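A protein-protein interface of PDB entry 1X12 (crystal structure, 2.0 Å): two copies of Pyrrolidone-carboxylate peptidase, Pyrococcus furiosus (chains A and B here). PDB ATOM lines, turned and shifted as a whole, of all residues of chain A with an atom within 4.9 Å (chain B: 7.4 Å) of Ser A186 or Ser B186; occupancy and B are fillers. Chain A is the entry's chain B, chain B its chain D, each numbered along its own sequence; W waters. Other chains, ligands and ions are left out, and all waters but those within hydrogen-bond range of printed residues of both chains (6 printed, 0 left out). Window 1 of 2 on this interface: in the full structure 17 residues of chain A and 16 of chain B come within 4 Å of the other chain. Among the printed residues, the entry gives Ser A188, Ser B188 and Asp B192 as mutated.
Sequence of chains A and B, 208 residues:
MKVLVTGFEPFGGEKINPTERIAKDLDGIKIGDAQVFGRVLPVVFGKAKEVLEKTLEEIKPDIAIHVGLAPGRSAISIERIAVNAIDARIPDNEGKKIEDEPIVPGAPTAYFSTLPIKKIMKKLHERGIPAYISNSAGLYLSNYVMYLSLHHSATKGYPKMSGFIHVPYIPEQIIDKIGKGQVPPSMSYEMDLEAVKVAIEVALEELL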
ATOM      1  N   SER A  74      11.328 -17.337 -36.446  1.00  0.00           N
ATOM      2  CA  SER A  74      11.122 -17.932 -35.128  1.00  0.00           C
ATOM      3  C   SER A  74      12.261 -17.833 -34.124  1.00  0.00           C
ATOM      4  O   SER A  74      12.095 -18.210 -32.961  1.00  0.00           O
ATOM      5  CB  SER A  74      10.767 -19.404 -35.307  1.00  0.00           C
ATOM      6  OG  SER A  74      11.829 -20.062 -35.975  1.00  0.00           O
ATOM      7  N   PRO A 130      17.966 -19.534 -28.972  1.00  0.00           N
ATOM      8  CA  PRO A 130      17.953 -20.116 -30.317  1.00  0.00           C
ATOM      9  C   PRO A 130      18.356 -19.064 -31.345  1.00  0.00           C
ATOM     10  O   PRO A 130      17.834 -17.948 -31.352  1.00  0.00           O
ATOM     11  CB  PRO A 130      16.510 -20.595 -30.480  1.00  0.00           C
ATOM     12  CG  PRO A 130      15.739 -19.700 -29.569  1.00  0.00           C
ATOM     13  CD  PRO A 130      16.626 -19.570 -28.364  1.00  0.00           C
ATOM     14  N   PRO A 168      12.685 -11.793 -34.104  1.00  0.00           N
ATOM     15  CA  PRO A 168      11.290 -12.118 -34.420  1.00  0.00           C
ATOM     16  C   PRO A 168      10.368 -11.063 -33.811  1.00  0.00           C
ATOM     17  O   PRO A 168      10.825 -10.140 -33.131  1.00  0.00           O
ATOM     18  CB  PRO A 168      11.078 -13.470 -33.733  1.00  0.00           C
ATOM     19  CG  PRO A 168      12.469 -14.040 -33.600  1.00  0.00           C
ATOM     20  CD  PRO A 168      13.287 -12.828 -33.244  1.00  0.00           C
ATOM     21  N   TYR A 169       9.070 -11.199 -34.062  1.00  0.00           N
ATOM     22  CA  TYR A 169       8.097 -10.305 -33.454  1.00  0.00           C
ATOM     23  C   TYR A 169       8.236 -10.584 -31.962  1.00  0.00           C
ATOM     24  O   TYR A 169       8.664 -11.676 -31.580  1.00  0.00           O
ATOM     25  CB  TYR A 169       6.666 -10.724 -33.798  1.00  0.00           C
ATOM     26  CG  TYR A 169       6.119 -10.337 -35.149  1.00  0.00           C
ATOM     27  CD1 TYR A 169       5.979  -9.000 -35.513  1.00  0.00           C
ATOM     28  CD2 TYR A 169       5.641 -11.315 -36.023  1.00  0.00           C
ATOM     29  CE1 TYR A 169       5.362  -8.643 -36.721  1.00  0.00           C
ATOM     30  CE2 TYR A 169       5.026 -10.970 -37.225  1.00  0.00           C
ATOM     31  CZ  TYR A 169       4.889  -9.639 -37.566  1.00  0.00           C
ATOM     32  OH  TYR A 169       4.264  -9.311 -38.748  1.00  0.00           O
ATOM     33  N   ILE A 170       7.888  -9.617 -31.117  1.00  0.00           N
ATOM     34  CA  ILE A 170       7.886  -9.884 -29.688  1.00  0.00           C
ATOM     35  C   ILE A 170       6.415 -10.268 -29.457  1.00  0.00           C
ATOM     36  O   ILE A 170       5.538  -9.860 -30.222  1.00  0.00           O
ATOM     37  CB  ILE A 170       8.291  -8.655 -28.832  1.00  0.00           C
ATOM     38  CG1 ILE A 170       7.463  -7.433 -29.212  1.00  0.00           C
ATOM     39  CG2 ILE A 170       9.786  -8.388 -28.991  1.00  0.00           C
ATOM     40  CD1 ILE A 170       7.739  -6.235 -28.309  1.00  0.00           C
ATOM     41  N   PRO A 171       6.129 -11.063 -28.416  1.00  0.00           N
ATOM     42  CA  PRO A 171       4.768 -11.516 -28.102  1.00  0.00           C
ATOM     43  C   PRO A 171       3.608 -10.529 -28.243  1.00  0.00           C
ATOM     44  O   PRO A 171       2.578 -10.865 -28.834  1.00  0.00           O
ATOM     45  CB  PRO A 171       4.908 -12.046 -26.679  1.00  0.00           C
ATOM     46  CG  PRO A 171       6.297 -12.613 -26.697  1.00  0.00           C
ATOM     47  CD  PRO A 171       7.076 -11.523 -27.385  1.00  0.00           C
ATOM     48  N   ILE A 174       1.918 -10.083 -31.553  1.00  0.00           N
ATOM     49  CA  ILE A 174       1.137 -11.193 -32.083  1.00  0.00           C
ATOM     50  C   ILE A 174      -0.360 -11.095 -31.763  1.00  0.00           C
ATOM     51  O   ILE A 174      -1.194 -11.630 -32.499  1.00  0.00           O
ATOM     52  CB  ILE A 174       1.666 -12.547 -31.541  1.00  0.00           C
ATOM     53  CG1 ILE A 174       3.165 -12.692 -31.836  1.00  0.00           C
ATOM     54  CG2 ILE A 174       0.892 -13.698 -32.168  1.00  0.00           C
ATOM     55  CD1 ILE A 174       3.515 -12.654 -33.305  1.00  0.00           C
ATOM     56  N   PRO A 184       1.940 -15.973 -35.936  1.00  0.00           N
ATOM     57  CA  PRO A 184       3.378 -15.956 -36.232  1.00  0.00           C
ATOM     58  C   PRO A 184       4.198 -16.246 -34.978  1.00  0.00           C
ATOM     59  O   PRO A 184       3.739 -16.019 -33.858  1.00  0.00           O
ATOM     60  CB  PRO A 184       3.621 -14.528 -36.723  1.00  0.00           C
ATOM     61  CG  PRO A 184       2.311 -14.123 -37.293  1.00  0.00           C
ATOM     62  CD  PRO A 184       1.327 -14.679 -36.286  1.00  0.00           C
ATOM     63  N   PRO A 185       5.426 -16.754 -35.156  1.00  0.00           N
ATOM     64  CA  PRO A 185       6.311 -17.063 -34.031  1.00  0.00           C
ATOM     65  C   PRO A 185       6.709 -15.742 -33.373  1.00  0.00           C
ATOM     66  O   PRO A 185       6.628 -14.682 -34.002  1.00  0.00           O
ATOM     67  CB  PRO A 185       7.516 -17.726 -34.705  1.00  0.00           C
ATOM     68  CG  PRO A 185       6.958 -18.269 -35.988  1.00  0.00           C
ATOM     69  CD  PRO A 185       6.029 -17.178 -36.431  1.00  0.00           C
ATOM     70  N   SER A 186       7.133 -15.806 -32.116  1.00  0.00           N
ATOM     71  CA  SER A 186       7.570 -14.615 -31.399  1.00  0.00           C
ATOM     72  C   SER A 186       8.677 -14.983 -30.416  1.00  0.00           C
ATOM     73  O   SER A 186       8.889 -16.161 -30.116  1.00  0.00           O
ATOM     74  CB  SER A 186       6.395 -13.965 -30.654  1.00  0.00           C
ATOM     75  OG  SER A 186       5.822 -14.847 -29.703  1.00  0.00           O
ATOM     76  N   MET A 187       9.388 -13.969 -29.931  1.00  0.00           N
ATOM     77  CA  MET A 187      10.478 -14.161 -28.979  1.00  0.00           C
ATOM     78  C   MET A 187      10.480 -12.953 -28.046  1.00  0.00           C
ATOM     79  O   MET A 187      10.265 -11.825 -28.483  1.00  0.00           O
ATOM     80  CB  MET A 187      11.815 -14.279 -29.721  1.00  0.00           C
ATOM     81  CG  MET A 187      13.012 -14.520 -28.808  1.00  0.00           C
ATOM     82  SD  MET A 187      14.485 -14.977 -29.735  1.00  0.00           S
ATOM     83  CE  MET A 187      14.230 -16.746 -29.928  1.00  0.00           C
ATOM     84  N   SER A 188      10.714 -13.188 -26.760  1.00  0.00           N
ATOM     85  CA  SER A 188      10.684 -12.108 -25.781  1.00  0.00           C
ATOM     86  C   SER A 188      11.679 -10.991 -26.062  1.00  0.00           C
ATOM     87  O   SER A 188      12.761 -11.220 -26.601  1.00  0.00           O
ATOM     88  CB  SER A 188      10.947 -12.648 -24.371  1.00  0.00           C
ATOM     89  OG  SER A 188      12.325 -12.926 -24.186  1.00  0.00           O
ATOM     90  N   GLY B  72       5.997 -27.256 -32.087  1.00  0.00           N
ATOM     91  CA  GLY B  72       5.653 -26.571 -33.317  1.00  0.00           C
ATOM     92  C   GLY B  72       4.648 -25.439 -33.193  1.00  0.00           C
ATOM     93  O   GLY B  72       4.633 -24.545 -34.032  1.00  0.00           O
ATOM     94  N   ARG B  73       3.791 -25.469 -32.178  1.00  0.00           N
ATOM     95  CA  ARG B  73       2.826 -24.385 -32.022  1.00  0.00           C
ATOM     96  C   ARG B  73       3.563 -23.123 -31.581  1.00  0.00           C
ATOM     97  O   ARG B  73       4.540 -23.197 -30.837  1.00  0.00           O
ATOM     98  CB  ARG B  73       1.718 -24.778 -31.033  1.00  0.00           C
ATOM     99  CG  ARG B  73       0.879 -25.958 -31.547  1.00  0.00           C
ATOM    100  CD  ARG B  73      -0.438 -26.130 -30.796  1.00  0.00           C
ATOM    101  NE  ARG B  73      -1.188 -27.279 -31.292  1.00  0.00           N
ATOM    102  CZ  ARG B  73      -2.367 -27.675 -30.820  1.00  0.00           C
ATOM    103  NH1 ARG B  73      -2.949 -27.014 -29.830  1.00  0.00           N
ATOM    104  NH2 ARG B  73      -2.963 -28.745 -31.335  1.00  0.00           N
ATOM    105  N   SER B  74       3.086 -21.972 -32.051  1.00  0.00           N
ATOM    106  CA  SER B  74       3.730 -20.685 -31.782  1.00  0.00           C
ATOM    107  C   SER B  74       3.175 -19.845 -30.640  1.00  0.00           C
ATOM    108  O   SER B  74       3.761 -18.823 -30.282  1.00  0.00           O
ATOM    109  CB  SER B  74       3.700 -19.841 -33.056  1.00  0.00           C
ATOM    110  OG  SER B  74       2.354 -19.627 -33.449  1.00  0.00           O
ATOM    111  N   ALA B  75       2.046 -20.252 -30.076  1.00  0.00           N
ATOM    112  CA  ALA B  75       1.460 -19.499 -28.976  1.00  0.00           C
ATOM    113  C   ALA B  75       0.661 -20.422 -28.080  1.00  0.00           C
ATOM    114  O   ALA B  75       0.506 -21.608 -28.375  1.00  0.00           O
ATOM    115  CB  ALA B  75       0.554 -18.393 -29.523  1.00  0.00           C
ATOM    116  N   PRO B 130       0.024 -14.017 -26.367  1.00  0.00           N
ATOM    117  CA  PRO B 130      -0.643 -14.541 -27.561  1.00  0.00           C
ATOM    118  C   PRO B 130      -1.243 -15.910 -27.259  1.00  0.00           C
ATOM    119  O   PRO B 130      -0.578 -16.792 -26.709  1.00  0.00           O
ATOM    120  CB  PRO B 130       0.481 -14.591 -28.602  1.00  0.00           C
ATOM    121  CG  PRO B 130       1.715 -14.729 -27.783  1.00  0.00           C
ATOM    122  CD  PRO B 130       1.465 -13.822 -26.603  1.00  0.00           C
ATOM    123  N   PRO B 168       3.906 -23.985 -26.280  1.00  0.00           N
ATOM    124  CA  PRO B 168       4.942 -24.239 -27.283  1.00  0.00           C
ATOM    125  C   PRO B 168       6.210 -24.735 -26.594  1.00  0.00           C
ATOM    126  O   PRO B 168       6.264 -24.833 -25.366  1.00  0.00           O
ATOM    127  CB  PRO B 168       5.174 -22.861 -27.908  1.00  0.00           C
ATOM    128  CG  PRO B 168       3.904 -22.110 -27.629  1.00  0.00           C
ATOM    129  CD  PRO B 168       3.552 -22.555 -26.236  1.00  0.00           C
ATOM    130  N   TYR B 169       7.224 -25.060 -27.385  1.00  0.00           N
ATOM    131  CA  TYR B 169       8.512 -25.455 -26.826  1.00  0.00           C
ATOM    132  C   TYR B 169       8.981 -24.205 -26.094  1.00  0.00           C
ATOM    133  O   TYR B 169       8.568 -23.100 -26.452  1.00  0.00           O
ATOM    134  CB  TYR B 169       9.553 -25.670 -27.927  1.00  0.00           C
ATOM    135  CG  TYR B 169       9.524 -26.972 -28.683  1.00  0.00           C
ATOM    136  CD1 TYR B 169       9.736 -28.188 -28.031  1.00  0.00           C
ATOM    137  CD2 TYR B 169       9.393 -26.979 -30.075  1.00  0.00           C
ATOM    138  CE1 TYR B 169       9.826 -29.385 -28.753  1.00  0.00           C
ATOM    139  CE2 TYR B 169       9.483 -28.160 -30.802  1.00  0.00           C
ATOM    140  CZ  TYR B 169       9.702 -29.356 -30.139  1.00  0.00           C
ATOM    141  OH  TYR B 169       9.816 -30.515 -30.870  1.00  0.00           O
ATOM    142  N   ILE B 170       9.833 -24.362 -25.086  1.00  0.00           N
ATOM    143  CA  ILE B 170      10.402 -23.191 -24.435  1.00  0.00           C
ATOM    144  C   ILE B 170      11.731 -23.042 -25.189  1.00  0.00           C
ATOM    145  O   ILE B 170      12.258 -24.022 -25.730  1.00  0.00           O
ATOM    146  CB  ILE B 170      10.636 -23.382 -22.908  1.00  0.00           C
ATOM    147  CG1 ILE B 170      11.429 -24.656 -22.633  1.00  0.00           C
ATOM    148  CG2 ILE B 170       9.288 -23.385 -22.178  1.00  0.00           C
ATOM    149  CD1 ILE B 170      11.790 -24.827 -21.167  1.00  0.00           C
ATOM    150  N   PRO B 171      12.283 -21.822 -25.252  1.00  0.00           N
ATOM    151  CA  PRO B 171      13.540 -21.547 -25.956  1.00  0.00           C
ATOM    152  C   PRO B 171      14.684 -22.557 -25.851  1.00  0.00           C
ATOM    153  O   PRO B 171      15.270 -22.924 -26.868  1.00  0.00           O
ATOM    154  CB  PRO B 171      13.931 -20.173 -25.427  1.00  0.00           C
ATOM    155  CG  PRO B 171      12.594 -19.518 -25.240  1.00  0.00           C
ATOM    156  CD  PRO B 171      11.808 -20.612 -24.555  1.00  0.00           C
ATOM    157  N   GLU B 172      15.007 -23.003 -24.641  1.00  0.00           N
ATOM    158  CA  GLU B 172      16.108 -23.948 -24.468  1.00  0.00           C
ATOM    159  C   GLU B 172      15.926 -25.258 -25.228  1.00  0.00           C
ATOM    160  O   GLU B 172      16.904 -25.933 -25.552  1.00  0.00           O
ATOM    161  CB  GLU B 172      16.344 -24.229 -22.977  1.00  0.00           C
ATOM    162  CG  GLU B 172      15.110 -24.640 -22.208  1.00  0.00           C
ATOM    163  CD  GLU B 172      15.355 -24.671 -20.712  1.00  0.00           C
ATOM    164  OE1 GLU B 172      15.899 -25.682 -20.222  1.00  0.00           O
ATOM    165  OE2 GLU B 172      15.012 -23.677 -20.031  1.00  0.00           O
ATOM    166  N   GLN B 173      14.681 -25.610 -25.527  1.00  0.00           N
ATOM    167  CA  GLN B 173      14.388 -26.842 -26.249  1.00  0.00           C
ATOM    168  C   GLN B 173      14.661 -26.712 -27.740  1.00  0.00           C
ATOM    169  O   GLN B 173      14.704 -27.713 -28.459  1.00  0.00           O
ATOM    170  CB  GLN B 173      12.925 -27.239 -26.056  1.00  0.00           C
ATOM    171  CG  GLN B 173      12.567 -27.638 -24.640  1.00  0.00           C
ATOM    172  CD  GLN B 173      11.128 -28.092 -24.537  1.00  0.00           C
ATOM    173  OE1 GLN B 173      10.203 -27.280 -24.619  1.00  0.00           O
ATOM    174  NE2 GLN B 173      10.928 -29.399 -24.378  1.00  0.00           N
ATOM    175  N   ILE B 174      14.833 -25.478 -28.202  1.00  0.00           N
ATOM    176  CA  ILE B 174      15.091 -25.210 -29.611  1.00  0.00           C
ATOM    177  C   ILE B 174      16.572 -25.340 -29.995  1.00  0.00           C
ATOM    178  O   ILE B 174      16.891 -25.633 -31.144  1.00  0.00           O
ATOM    179  CB  ILE B 174      14.612 -23.784 -29.992  1.00  0.00           C
ATOM    180  CG1 ILE B 174      13.136 -23.605 -29.620  1.00  0.00           C
ATOM    181  CG2 ILE B 174      14.816 -23.541 -31.482  1.00  0.00           C
ATOM    182  CD1 ILE B 174      12.195 -24.566 -30.325  1.00  0.00           C
ATOM    183  N   VAL B 183      13.962 -24.469 -37.224  1.00  0.00           N
ATOM    184  CA  VAL B 183      13.866 -23.650 -36.028  1.00  0.00           C
ATOM    185  C   VAL B 183      12.396 -23.455 -35.661  1.00  0.00           C
ATOM    186  O   VAL B 183      11.736 -22.531 -36.144  1.00  0.00           O
ATOM    187  CB  VAL B 183      14.541 -22.277 -36.236  1.00  0.00           C
ATOM    188  CG1 VAL B 183      14.646 -21.548 -34.908  1.00  0.00           C
ATOM    189  CG2 VAL B 183      15.926 -22.462 -36.852  1.00  0.00           C
ATOM    190  N   PRO B 184      11.860 -24.354 -34.817  1.00  0.00           N
ATOM    191  CA  PRO B 184      10.466 -24.296 -34.366  1.00  0.00           C
ATOM    192  C   PRO B 184      10.226 -23.074 -33.482  1.00  0.00           C
ATOM    193  O   PRO B 184      11.154 -22.553 -32.863  1.00  0.00           O
ATOM    194  CB  PRO B 184      10.303 -25.587 -33.559  1.00  0.00           C
ATOM    195  CG  PRO B 184      11.295 -26.512 -34.172  1.00  0.00           C
ATOM    196  CD  PRO B 184      12.494 -25.609 -34.376  1.00  0.00           C
ATOM    197  N   PRO B 185       8.972 -22.603 -33.418  1.00  0.00           N
ATOM    198  CA  PRO B 185       8.614 -21.445 -32.596  1.00  0.00           C
ATOM    199  C   PRO B 185       8.785 -21.842 -31.132  1.00  0.00           C
ATOM    200  O   PRO B 185       8.777 -23.030 -30.808  1.00  0.00           O
ATOM    201  CB  PRO B 185       7.137 -21.219 -32.930  1.00  0.00           C
ATOM    202  CG  PRO B 185       6.973 -21.833 -34.288  1.00  0.00           C
ATOM    203  CD  PRO B 185       7.805 -23.081 -34.181  1.00  0.00           C
ATOM    204  N   SER B 186       8.941 -20.858 -30.256  1.00  0.00           N
ATOM    205  CA  SER B 186       9.080 -21.121 -28.834  1.00  0.00           C
ATOM    206  C   SER B 186       8.450 -19.975 -28.040  1.00  0.00           C
ATOM    207  O   SER B 186       8.170 -18.910 -28.592  1.00  0.00           O
ATOM    208  CB  SER B 186      10.560 -21.281 -28.452  1.00  0.00           C
ATOM    209  OG  SER B 186      11.308 -20.112 -28.745  1.00  0.00           O
ATOM    210  N   MET B 187       8.211 -20.212 -26.755  1.00  0.00           N
ATOM    211  CA  MET B 187       7.625 -19.207 -25.871  1.00  0.00           C
ATOM    212  C   MET B 187       8.255 -19.410 -24.493  1.00  0.00           C
ATOM    213  O   MET B 187       8.468 -20.543 -24.070  1.00  0.00           O
ATOM    214  CB  MET B 187       6.105 -19.386 -25.805  1.00  0.00           C
ATOM    215  CG  MET B 187       5.387 -18.362 -24.927  1.00  0.00           C
ATOM    216  SD  MET B 187       3.595 -18.399 -25.166  1.00  0.00           S
ATOM    217  CE  MET B 187       3.430 -17.347 -26.606  1.00  0.00           C
ATOM    218  N   SER B 188       8.557 -18.318 -23.801  1.00  0.00           N
ATOM    219  CA  SER B 188       9.199 -18.413 -22.492  1.00  0.00           C
ATOM    220  C   SER B 188       8.396 -19.205 -21.473  1.00  0.00           C
ATOM    221  O   SER B 188       7.159 -19.225 -21.509  1.00  0.00           O
ATOM    222  CB  SER B 188       9.469 -17.015 -21.923  1.00  0.00           C
ATOM    223  OG  SER B 188       8.281 -16.455 -21.396  1.00  0.00           O
ATOM    224  N   MET B 191       6.112 -16.963 -19.393  1.00  0.00           N
ATOM    225  CA  MET B 191       4.837 -16.605 -20.003  1.00  0.00           C
ATOM    226  C   MET B 191       3.845 -17.758 -19.876  1.00  0.00           C
ATOM    227  O   MET B 191       2.662 -17.536 -19.623  1.00  0.00           O
ATOM    228  CB  MET B 191       5.021 -16.244 -21.478  1.00  0.00           C
ATOM    229  CG  MET B 191       3.720 -15.868 -22.166  1.00  0.00           C
ATOM    230  SD  MET B 191       3.970 -15.052 -23.753  1.00  0.00           S
ATOM    231  CE  MET B 191       4.347 -13.378 -23.186  1.00  0.00           C
ATOM    232  N   ASP B 192       4.336 -18.984 -20.066  1.00  0.00           N
ATOM    233  CA  ASP B 192       3.498 -20.178 -19.954  1.00  0.00           C
ATOM    234  C   ASP B 192       2.894 -20.274 -18.556  1.00  0.00           C
ATOM    235  O   ASP B 192       1.694 -20.494 -18.403  1.00  0.00           O
ATOM    236  CB  ASP B 192       4.312 -21.451 -20.208  1.00  0.00           C
ATOM    237  CG  ASP B 192       4.794 -21.574 -21.645  1.00  0.00           C
ATOM    238  OD1 ASP B 192       4.266 -20.874 -22.529  1.00  0.00           O
ATOM    239  OD2 ASP B 192       5.702 -22.398 -21.893  1.00  0.00           O
HETATM  240  O   HOH W   1      12.313 -20.685 -31.451  1.00  0.00           O
HETATM  241  O   HOH W   2      10.782 -17.552 -28.361  1.00  0.00           O
HETATM  242  O   HOH W   3       6.926 -16.482 -27.782  1.00  0.00           O
HETATM  243  O   HOH W   4       3.769 -16.159 -31.087  1.00  0.00           O
HETATM  244  O   HOH W   5       9.556 -18.438 -31.824  1.00  0.00           O
HETATM  245  O   HOH W   6       6.445 -18.393 -30.902  1.00  0.00           O
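Hydrophobic or aromatic side chains of chain A that line the printed part of chain B: Pro A130, Pro A171, Ile A174 and Pro A185.
Among the printed residues, no Asp or Glu carboxylate lies within 4 Å of a Lys or Arg side-chain nitrogen of the other chain.
Water W1 lies within hydrogen-bond range of the backbone carbonyl oxygen of Pro B184 (2.6 Å), the backbone carbonyl oxygen of Ser A74 (2.9 Å) and the side-chain hydroxyl of Ser B186 (2.9 Å).
Water W2 bridges OG of Ser B186 (2.6 Å) and O of Ser A186 (2.9 Å).
Water W3 bridges the side-chain hydroxyl (OG) of Ser A186 (2.8 Å) and the backbone carbonyl oxygen (O) of Ser B186 (2.8 Å).
Water W4 lies within hydrogen-bond range of O of Pro A184 (2.8 Å), O of Ser B74 (2.8 Å) and OG of Ser A186 (2.8 Å).
Water W6 lies within hydrogen-bond range of the backbone carbonyl oxygen of Ser B74 (2.8 Å), the backbone carbonyl oxygen of Ser B186 (2.9 Å) and the backbone NH of Ser A186 (2.9 Å).
Water W5 lies within hydrogen-bond range of the backbone carbonyl oxygen (O) of Ser A74 (2.8 Å), the backbone carbonyl oxygen (O) of Ser A186 (2.9 Å) and the backbone NH (N) of Ser B186 (2.9 Å).
Pro A130 touches Pro B171, and with the chains exchanged Pro A171 touches Pro B130.
Pro A184 touches Ser B74, but with the chains exchanged Ser A74 does not touch Pro B184 (4.005 Å).
Pro A185 touches its own counterpart, Pro B185.
Ser A186 touches its own counterpart, Ser B186.
Positions printed for both chains: 74, 130, 168, 169, 170, 171, 174, 184, 185, 186, 187 and 188.
Among the printed residues, merely in contact across the chains: Pro A130 with Pro B171 (3.9 Å), Pro A130 with Ile B174 (3.5 Å), Pro A171 with Pro B130 (3.9 Å), Pro A171 with Met B191 (3.8 Å), Ile A174 with Pro B130 (3.7 Å), Pro A184 with Ser B74 (3.9 Å), Pro A185 with Ser B74 (3.9 Å) and Pro A185 with Pro B185 (3.9 Å).
O of Val B183 sits at hydrogen-bond distance from OG of Ser A74 (2.5 Å).
The backbone carbonyl oxygen of Ser A186 sits close to the backbone carbonyl oxygen of Ser B186 (3.2 Å).
Of chain A, only Ser A186 comes within 4 Å of Ser B186.
Of the printed residues of chain A, Pro B130 touches Pro A171 (3.9 Å) and Ile A174 (3.7 Å).
Printed residues of chain B within 4 Å of Ile A174: Pro B130.
Of the printed residues of chain B, Pro A184 touches Ser B74 (3.9 Å).
Printed residues of chain B within 4 Å of Ser A74: Val B183 (2.5 Å).
Of the printed residues of chain B, Pro A185 touches Ser B74 (3.9 Å) and Pro B185 (3.9 Å).
The nearest printed residue of chain B that does not touch Ser A186 is Ser B74 (4.5 Å).
The nearest residue of chain A that does not touch Ser B186 is Pro A130 (4.5 Å).
The nearest printed residue of chain B that does not touch Ser A74 is Pro B184 (4.005 Å).
OG of Ser B188 lies within hydrogen-bond range of N of Met B191, 3.0 Å away.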
